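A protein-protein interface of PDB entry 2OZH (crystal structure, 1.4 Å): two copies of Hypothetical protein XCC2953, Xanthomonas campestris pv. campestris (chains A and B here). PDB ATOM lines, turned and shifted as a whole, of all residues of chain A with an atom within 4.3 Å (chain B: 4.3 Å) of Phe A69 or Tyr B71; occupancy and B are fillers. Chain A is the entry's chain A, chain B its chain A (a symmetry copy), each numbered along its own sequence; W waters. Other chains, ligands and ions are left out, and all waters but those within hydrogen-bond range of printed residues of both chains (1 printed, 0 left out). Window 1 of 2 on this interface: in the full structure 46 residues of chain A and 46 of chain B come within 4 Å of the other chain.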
ATOM      1  N   ILE A  63       0.125 -25.865  23.754  1.00  0.00           N
ATOM      2  CA  ILE A  63      -0.009 -25.289  22.430  1.00  0.00           C
ATOM      3  C   ILE A  63      -0.821 -23.997  22.642  1.00  0.00           C
ATOM      4  O   ILE A  63      -1.923 -24.053  23.168  1.00  0.00           O
ATOM      5  CB  ILE A  63      -0.749 -26.225  21.485  1.00  0.00           C
ATOM      6  CG1 ILE A  63      -0.012 -27.566  21.402  1.00  0.00           C
ATOM      7  CG2 ILE A  63      -0.860 -25.599  20.111  1.00  0.00           C
ATOM      8  CD1 ILE A  63      -0.783 -28.626  20.641  1.00  0.00           C
ATOM      9  N   SER A  64      -0.294 -22.866  22.202  1.00  0.00           N
ATOM     10  CA  SER A  64      -0.932 -21.585  22.506  1.00  0.00           C
ATOM     11  C   SER A  64      -0.552 -20.527  21.514  1.00  0.00           C
ATOM     12  O   SER A  64       0.503 -20.605  20.885  1.00  0.00           O
ATOM     13  CB  SER A  64      -0.485 -21.147  23.892  1.00  0.00           C
ATOM     14  OG  SER A  64      -1.104 -19.929  24.327  1.00  0.00           O
ATOM     15  N   ASP A  65      -1.401 -19.498  21.404  1.00  0.00           N
ATOM     16  CA  ASP A  65      -1.047 -18.266  20.717  1.00  0.00           C
ATOM     17  C   ASP A  65      -0.415 -17.231  21.645  1.00  0.00           C
ATOM     18  O   ASP A  65      -0.122 -16.130  21.204  1.00  0.00           O
ATOM     19  CB  ASP A  65      -2.238 -17.685  19.976  1.00  0.00           C
ATOM     20  CG  ASP A  65      -3.334 -17.221  20.876  1.00  0.00           C
ATOM     21  OD1 ASP A  65      -3.238 -17.416  22.110  1.00  0.00           O
ATOM     22  OD2 ASP A  65      -4.295 -16.620  20.332  1.00  0.00           O
ATOM     23  N   ALA A  67      -1.720 -15.486  23.803  1.00  0.00           N
ATOM     24  CA  ALA A  67      -2.568 -14.308  23.791  1.00  0.00           C
ATOM     25  C   ALA A  67      -4.009 -14.534  24.201  1.00  0.00           C
ATOM     26  O   ALA A  67      -4.521 -13.796  25.052  1.00  0.00           O
ATOM     27  CB  ALA A  67      -2.523 -13.662  22.423  1.00  0.00           C
ATOM     28  N   THR A  68      -4.643 -15.551  23.624  1.00  0.00           N
ATOM     29  CA  THR A  68      -6.063 -15.800  23.810  1.00  0.00           C
ATOM     30  C   THR A  68      -6.429 -17.231  24.223  1.00  0.00           C
ATOM     31  O   THR A  68      -7.463 -17.419  24.840  1.00  0.00           O
ATOM     32  CB  THR A  68      -6.902 -15.449  22.570  1.00  0.00           C
ATOM     33  OG1 THR A  68      -6.667 -16.397  21.510  1.00  0.00           O
ATOM     34  CG2 THR A  68      -6.652 -14.023  22.120  1.00  0.00           C
ATOM     35  N   PHE A  69      -5.608 -18.216  23.857  1.00  0.00           N
ATOM     36  CA  PHE A  69      -5.972 -19.618  23.953  1.00  0.00           C
ATOM     37  C   PHE A  69      -4.754 -20.460  24.236  1.00  0.00           C
ATOM     38  O   PHE A  69      -3.677 -20.207  23.695  1.00  0.00           O
ATOM     39  CB  PHE A  69      -6.567 -20.106  22.624  1.00  0.00           C
ATOM     40  CG  PHE A  69      -6.845 -21.588  22.609  1.00  0.00           C
ATOM     41  CD1 PHE A  69      -8.032 -22.112  23.093  1.00  0.00           C
ATOM     42  CD2 PHE A  69      -5.894 -22.476  22.097  1.00  0.00           C
ATOM     43  CE1 PHE A  69      -8.235 -23.484  23.090  1.00  0.00           C
ATOM     44  CE2 PHE A  69      -6.117 -23.825  22.096  1.00  0.00           C
ATOM     45  CZ  PHE A  69      -7.293 -24.328  22.585  1.00  0.00           C
ATOM     46  N   ALA A  70      -4.926 -21.475  25.083  1.00  0.00           N
ATOM     47  CA  ALA A  70      -3.908 -22.517  25.252  1.00  0.00           C
ATOM     48  C   ALA A  70      -4.579 -23.864  25.441  1.00  0.00           C
ATOM     49  O   ALA A  70      -5.683 -23.947  25.970  1.00  0.00           O
ATOM     50  CB  ALA A  70      -3.006 -22.235  26.441  1.00  0.00           C
ATOM     51  N   TYR A  71      -3.838 -24.909  25.060  1.00  0.00           N
ATOM     52  CA  TYR A  71      -4.244 -26.295  25.223  1.00  0.00           C
ATOM     53  C   TYR A  71      -3.099 -27.039  25.897  1.00  0.00           C
ATOM     54  O   TYR A  71      -1.966 -26.940  25.445  1.00  0.00           O
ATOM     55  CB  TYR A  71      -4.564 -26.930  23.845  1.00  0.00           C
ATOM     56  CG  TYR A  71      -4.791 -28.419  23.881  1.00  0.00           C
ATOM     57  CD1 TYR A  71      -5.956 -28.966  24.381  1.00  0.00           C
ATOM     58  CD2 TYR A  71      -3.823 -29.252  23.435  1.00  0.00           C
ATOM     59  CE1 TYR A  71      -6.117 -30.371  24.420  1.00  0.00           C
ATOM     60  CE2 TYR A  71      -3.966 -30.640  23.482  1.00  0.00           C
ATOM     61  CZ  TYR A  71      -5.108 -31.160  23.960  1.00  0.00           C
ATOM     62  OH  TYR A  71      -5.211 -32.568  24.010  1.00  0.00           O
ATOM     63  N   LEU A 103      -5.308 -15.388  29.477  1.00  0.00           N
ATOM     64  CA  LEU A 103      -5.932 -16.092  28.391  1.00  0.00           C
ATOM     65  C   LEU A 103      -7.425 -16.207  28.597  1.00  0.00           C
ATOM     66  O   LEU A 103      -7.876 -16.427  29.729  1.00  0.00           O
ATOM     67  CB  LEU A 103      -5.334 -17.508  28.299  1.00  0.00           C
ATOM     68  CG  LEU A 103      -3.826 -17.632  28.106  1.00  0.00           C
ATOM     69  CD1 LEU A 103      -3.415 -19.087  28.089  1.00  0.00           C
ATOM     70  CD2 LEU A 103      -3.366 -16.960  26.810  1.00  0.00           C
ATOM     71  N   ARG A 105      -9.236 -18.685  27.247  1.00  0.00           N
ATOM     72  CA  ARG A 105      -9.535 -20.106  27.401  1.00  0.00           C
ATOM     73  C   ARG A 105      -8.266 -20.927  27.471  1.00  0.00           C
ATOM     74  O   ARG A 105      -7.380 -20.785  26.607  1.00  0.00           O
ATOM     75  CB  ARG A 105     -10.370 -20.612  26.230  1.00  0.00           C
ATOM     76  CG  ARG A 105     -11.044 -21.964  26.545  1.00  0.00           C
ATOM     77  CD  ARG A 105     -11.662 -22.612  25.348  1.00  0.00           C
ATOM     78  NE  ARG A 105     -12.616 -21.796  24.611  1.00  0.00           N
ATOM     79  CZ  ARG A 105     -13.931 -21.986  24.515  1.00  0.00           C
ATOM     80  NH1 ARG A 105     -14.610 -22.930  25.176  1.00  0.00           N
ATOM     81  NH2 ARG A 105     -14.568 -21.184  23.704  1.00  0.00           N
ATOM     82  N   SER A 107      -7.635 -25.003  27.724  1.00  0.00           N
ATOM     83  CA  SER A 107      -8.375 -26.260  27.579  1.00  0.00           C
ATOM     84  C   SER A 107      -7.492 -27.488  27.776  1.00  0.00           C
ATOM     85  O   SER A 107      -6.287 -27.429  27.575  1.00  0.00           O
ATOM     86  CB  SER A 107      -8.957 -26.336  26.170  1.00  0.00           C
ATOM     87  OG  SER A 107      -9.855 -25.253  25.920  1.00  0.00           O
ATOM     88  N   ARG B  61      -8.584 -18.300  11.818  1.00  0.00           N
ATOM     89  CA  ARG B  61      -7.343 -18.397  12.558  1.00  0.00           C
ATOM     90  C   ARG B  61      -7.198 -19.762  13.220  1.00  0.00           C
ATOM     91  O   ARG B  61      -8.145 -20.248  13.828  1.00  0.00           O
ATOM     92  CB  ARG B  61      -7.242 -17.293  13.614  1.00  0.00           C
ATOM     93  CG  ARG B  61      -5.874 -17.233  14.289  1.00  0.00           C
ATOM     94  CD  ARG B  61      -5.676 -15.939  15.045  1.00  0.00           C
ATOM     95  NE  ARG B  61      -6.564 -15.783  16.181  1.00  0.00           N
ATOM     96  CZ  ARG B  61      -6.270 -16.162  17.418  1.00  0.00           C
ATOM     97  NH1 ARG B  61      -5.162 -16.837  17.679  1.00  0.00           N
ATOM     98  NH2 ARG B  61      -7.076 -15.847  18.403  1.00  0.00           N
ATOM     99  N   VAL B  62      -6.030 -20.357  13.062  1.00  0.00           N
ATOM    100  CA  VAL B  62      -5.749 -21.675  13.607  1.00  0.00           C
ATOM    101  C   VAL B  62      -4.555 -21.609  14.563  1.00  0.00           C
ATOM    102  O   VAL B  62      -3.506 -21.076  14.221  1.00  0.00           O
ATOM    103  CB  VAL B  62      -5.497 -22.689  12.473  1.00  0.00           C
ATOM    104  CG1 VAL B  62      -5.118 -24.067  13.038  1.00  0.00           C
ATOM    105  CG2 VAL B  62      -6.703 -22.796  11.570  1.00  0.00           C
ATOM    106  N   ILE B  63      -4.700 -22.174  15.758  1.00  0.00           N
ATOM    107  CA  ILE B  63      -3.608 -22.325  16.701  1.00  0.00           C
ATOM    108  C   ILE B  63      -3.273 -23.828  16.679  1.00  0.00           C
ATOM    109  O   ILE B  63      -4.143 -24.647  16.938  1.00  0.00           O
ATOM    110  CB  ILE B  63      -4.017 -21.898  18.103  1.00  0.00           C
ATOM    111  CG1 ILE B  63      -4.496 -20.443  18.084  1.00  0.00           C
ATOM    112  CG2 ILE B  63      -2.851 -22.057  19.058  1.00  0.00           C
ATOM    113  CD1 ILE B  63      -5.108 -19.997  19.396  1.00  0.00           C
ATOM    114  N   PHE B  69      -2.478 -31.381  17.055  1.00  0.00           N
ATOM    115  CA  PHE B  69      -3.625 -30.649  17.561  1.00  0.00           C
ATOM    116  C   PHE B  69      -3.764 -29.328  16.849  1.00  0.00           C
ATOM    117  O   PHE B  69      -2.768 -28.662  16.563  1.00  0.00           O
ATOM    118  CB  PHE B  69      -3.446 -30.346  19.056  1.00  0.00           C
ATOM    119  CG  PHE B  69      -4.539 -29.472  19.618  1.00  0.00           C
ATOM    120  CD1 PHE B  69      -5.731 -30.004  20.081  1.00  0.00           C
ATOM    121  CD2 PHE B  69      -4.368 -28.086  19.683  1.00  0.00           C
ATOM    122  CE1 PHE B  69      -6.723 -29.162  20.562  1.00  0.00           C
ATOM    123  CE2 PHE B  69      -5.356 -27.274  20.166  1.00  0.00           C
ATOM    124  CZ  PHE B  69      -6.532 -27.815  20.613  1.00  0.00           C
ATOM    125  N   ALA B  70      -5.008 -28.941  16.566  1.00  0.00           N
ATOM    126  CA  ALA B  70      -5.306 -27.580  16.110  1.00  0.00           C
ATOM    127  C   ALA B  70      -6.618 -27.113  16.711  1.00  0.00           C
ATOM    128  O   ALA B  70      -7.508 -27.914  16.977  1.00  0.00           O
ATOM    129  CB  ALA B  70      -5.391 -27.500  14.595  1.00  0.00           C
ATOM    130  N   TYR B  71      -6.725 -25.787  16.840  1.00  0.00           N
ATOM    131  CA  TYR B  71      -7.921 -25.112  17.316  1.00  0.00           C
ATOM    132  C   TYR B  71      -8.261 -24.010  16.321  1.00  0.00           C
ATOM    133  O   TYR B  71      -7.392 -23.221  15.974  1.00  0.00           O
ATOM    134  CB  TYR B  71      -7.679 -24.511  18.724  1.00  0.00           C
ATOM    135  CG  TYR B  71      -8.783 -23.613  19.218  1.00  0.00           C
ATOM    136  CD1 TYR B  71      -9.988 -24.118  19.663  1.00  0.00           C
ATOM    137  CD2 TYR B  71      -8.605 -22.272  19.208  1.00  0.00           C
ATOM    138  CE1 TYR B  71     -11.007 -23.236  20.095  1.00  0.00           C
ATOM    139  CE2 TYR B  71      -9.609 -21.393  19.619  1.00  0.00           C
ATOM    140  CZ  TYR B  71     -10.774 -21.896  20.060  1.00  0.00           C
ATOM    141  OH  TYR B  71     -11.774 -20.977  20.449  1.00  0.00           O
ATOM    142  N   LEU B  72      -9.507 -23.962  15.877  1.00  0.00           N
ATOM    143  CA  LEU B  72     -10.013 -22.964  14.944  1.00  0.00           C
ATOM    144  C   LEU B  72     -10.803 -21.928  15.696  1.00  0.00           C
ATOM    145  O   LEU B  72     -11.660 -22.240  16.488  1.00  0.00           O
ATOM    146  CB  LEU B  72     -10.927 -23.660  13.940  1.00  0.00           C
ATOM    147  CG  LEU B  72     -11.605 -22.795  12.878  1.00  0.00           C
ATOM    148  CD1 LEU B  72     -10.562 -22.236  11.898  1.00  0.00           C
ATOM    149  CD2 LEU B  72     -12.715 -23.568  12.155  1.00  0.00           C
ATOM    150  N   GLY B  73     -10.580 -20.668  15.347  1.00  0.00           N
ATOM    151  CA  GLY B  73     -11.410 -19.578  15.855  1.00  0.00           C
ATOM    152  C   GLY B  73     -11.315 -18.335  14.994  1.00  0.00           C
ATOM    153  O   GLY B  73     -10.666 -18.308  13.957  1.00  0.00           O
ATOM    154  N   PHE B 106      -8.771 -31.747  15.992  1.00  0.00           N
ATOM    155  CA  PHE B 106      -9.001 -30.374  15.514  1.00  0.00           C
ATOM    156  C   PHE B 106     -10.270 -29.937  16.242  1.00  0.00           C
ATOM    157  O   PHE B 106     -11.322 -30.565  16.079  1.00  0.00           O
ATOM    158  CB  PHE B 106      -9.182 -30.362  13.999  1.00  0.00           C
ATOM    159  CG  PHE B 106      -8.796 -29.081  13.314  1.00  0.00           C
ATOM    160  CD1 PHE B 106      -9.014 -27.844  13.889  1.00  0.00           C
ATOM    161  CD2 PHE B 106      -8.220 -29.150  12.064  1.00  0.00           C
ATOM    162  CE1 PHE B 106      -8.624 -26.686  13.227  1.00  0.00           C
ATOM    163  CE2 PHE B 106      -7.831 -28.022  11.385  1.00  0.00           C
ATOM    164  CZ  PHE B 106      -8.064 -26.780  11.952  1.00  0.00           C
ATOM    165  N   SER B 107     -10.157 -28.900  17.057  1.00  0.00           N
ATOM    166  CA  SER B 107     -11.246 -28.455  17.932  1.00  0.00           C
ATOM    167  C   SER B 107     -11.747 -27.057  17.582  1.00  0.00           C
ATOM    168  O   SER B 107     -11.018 -26.258  17.012  1.00  0.00           O
ATOM    169  CB  SER B 107     -10.744 -28.414  19.372  1.00  0.00           C
ATOM    170  OG  SER B 107     -10.315 -29.705  19.809  1.00  0.00           O
ATOM    171  N   LEU B 108     -12.991 -26.790  17.952  1.00  0.00           N
ATOM    172  CA  LEU B 108     -13.576 -25.453  17.811  1.00  0.00           C
ATOM    173  C   LEU B 108     -14.742 -25.333  18.791  1.00  0.00           C
ATOM    174  O   LEU B 108     -15.212 -26.332  19.318  1.00  0.00           O
ATOM    175  CB  LEU B 108     -14.036 -25.207  16.385  1.00  0.00           C
ATOM    176  CG  LEU B 108     -15.147 -26.071  15.812  1.00  0.00           C
ATOM    177  CD1 LEU B 108     -16.529 -25.605  16.312  1.00  0.00           C
ATOM    178  CD2 LEU B 108     -15.082 -26.032  14.279  1.00  0.00           C
HETATM  179  O   HOH W   1     -11.422 -19.995  22.945  1.00  0.00           O
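The backbone carbonyl oxygen (O) of Ile A63 lies within hydrogen-bond range of the backbone NH (N) of Tyr A71. OG of Ser A64 lies within hydrogen-bond range of O of Phe A69. N of Ala A67 is in hydrogen-bond range of OD1 of Asp A65 (3.0 Å). OD2 of Asp A65 sits at hydrogen-bond distance from OG1 of Thr A68. O of Thr A68 sits at hydrogen-bond distance from N of Arg A105, 3.2 Å away. The backbone carbonyl oxygen (O) of Arg B61 is in hydrogen-bond range of the backbone NH (N) of Gly B73.
Hydrophobic or aromatic side chains of chain B within 4 Å of the printed part of chain A: Ile B63, Phe B69 and Tyr B71. Along chain A the printed residues that touch a printed residue of chain B span positions 63 to 71. Among the printed residues, 8 pairs touch across the chains.
Tyr B71 touches one residue of chain A. Printed residues of chain A within 4 Å of Arg B61: Asp A65 and Thr A68. Printed residues of chain B within 4 Å of Tyr A71: Phe B69. The nearest residue of chain B that does not touch Phe A69 is Phe B69 (4.02 Å).
Among the printed residues, pairs that only touch across the chains: Phe A69 with Ile B63 (3.5 Å), Ile A63 with Phe B69 (3.5 Å), Asp A65 with Ile B63 (3.6 Å), Ser A64 with Ile B63 (3.7 Å), Phe A69 with Tyr B71 (3.8 Å) and Tyr A71 with Phe B69 (3.8 Å).
Ile A63 touches Phe B69, and with the chains exchanged Phe A69 touches Ile B63. Phe A69 touches Tyr B71, and with the chains exchanged Tyr A71 touches Phe B69. Positions printed for both chains: 63, 69, 70, 71 and 107. Of the 8 pairs that touch across the chains among the printed residues, 4 have their exchanged pair printed and touching as well.
Water W1 bridges OH of Tyr B71 and NE of Arg A105.
The side-chain carboxylate (OD2) of Asp A65 is in salt-bridge range of the guanidinium group (NH1) of Arg B61. OG1 of Thr A68 sits at hydrogen-bond distance from NH2 of Arg B61.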
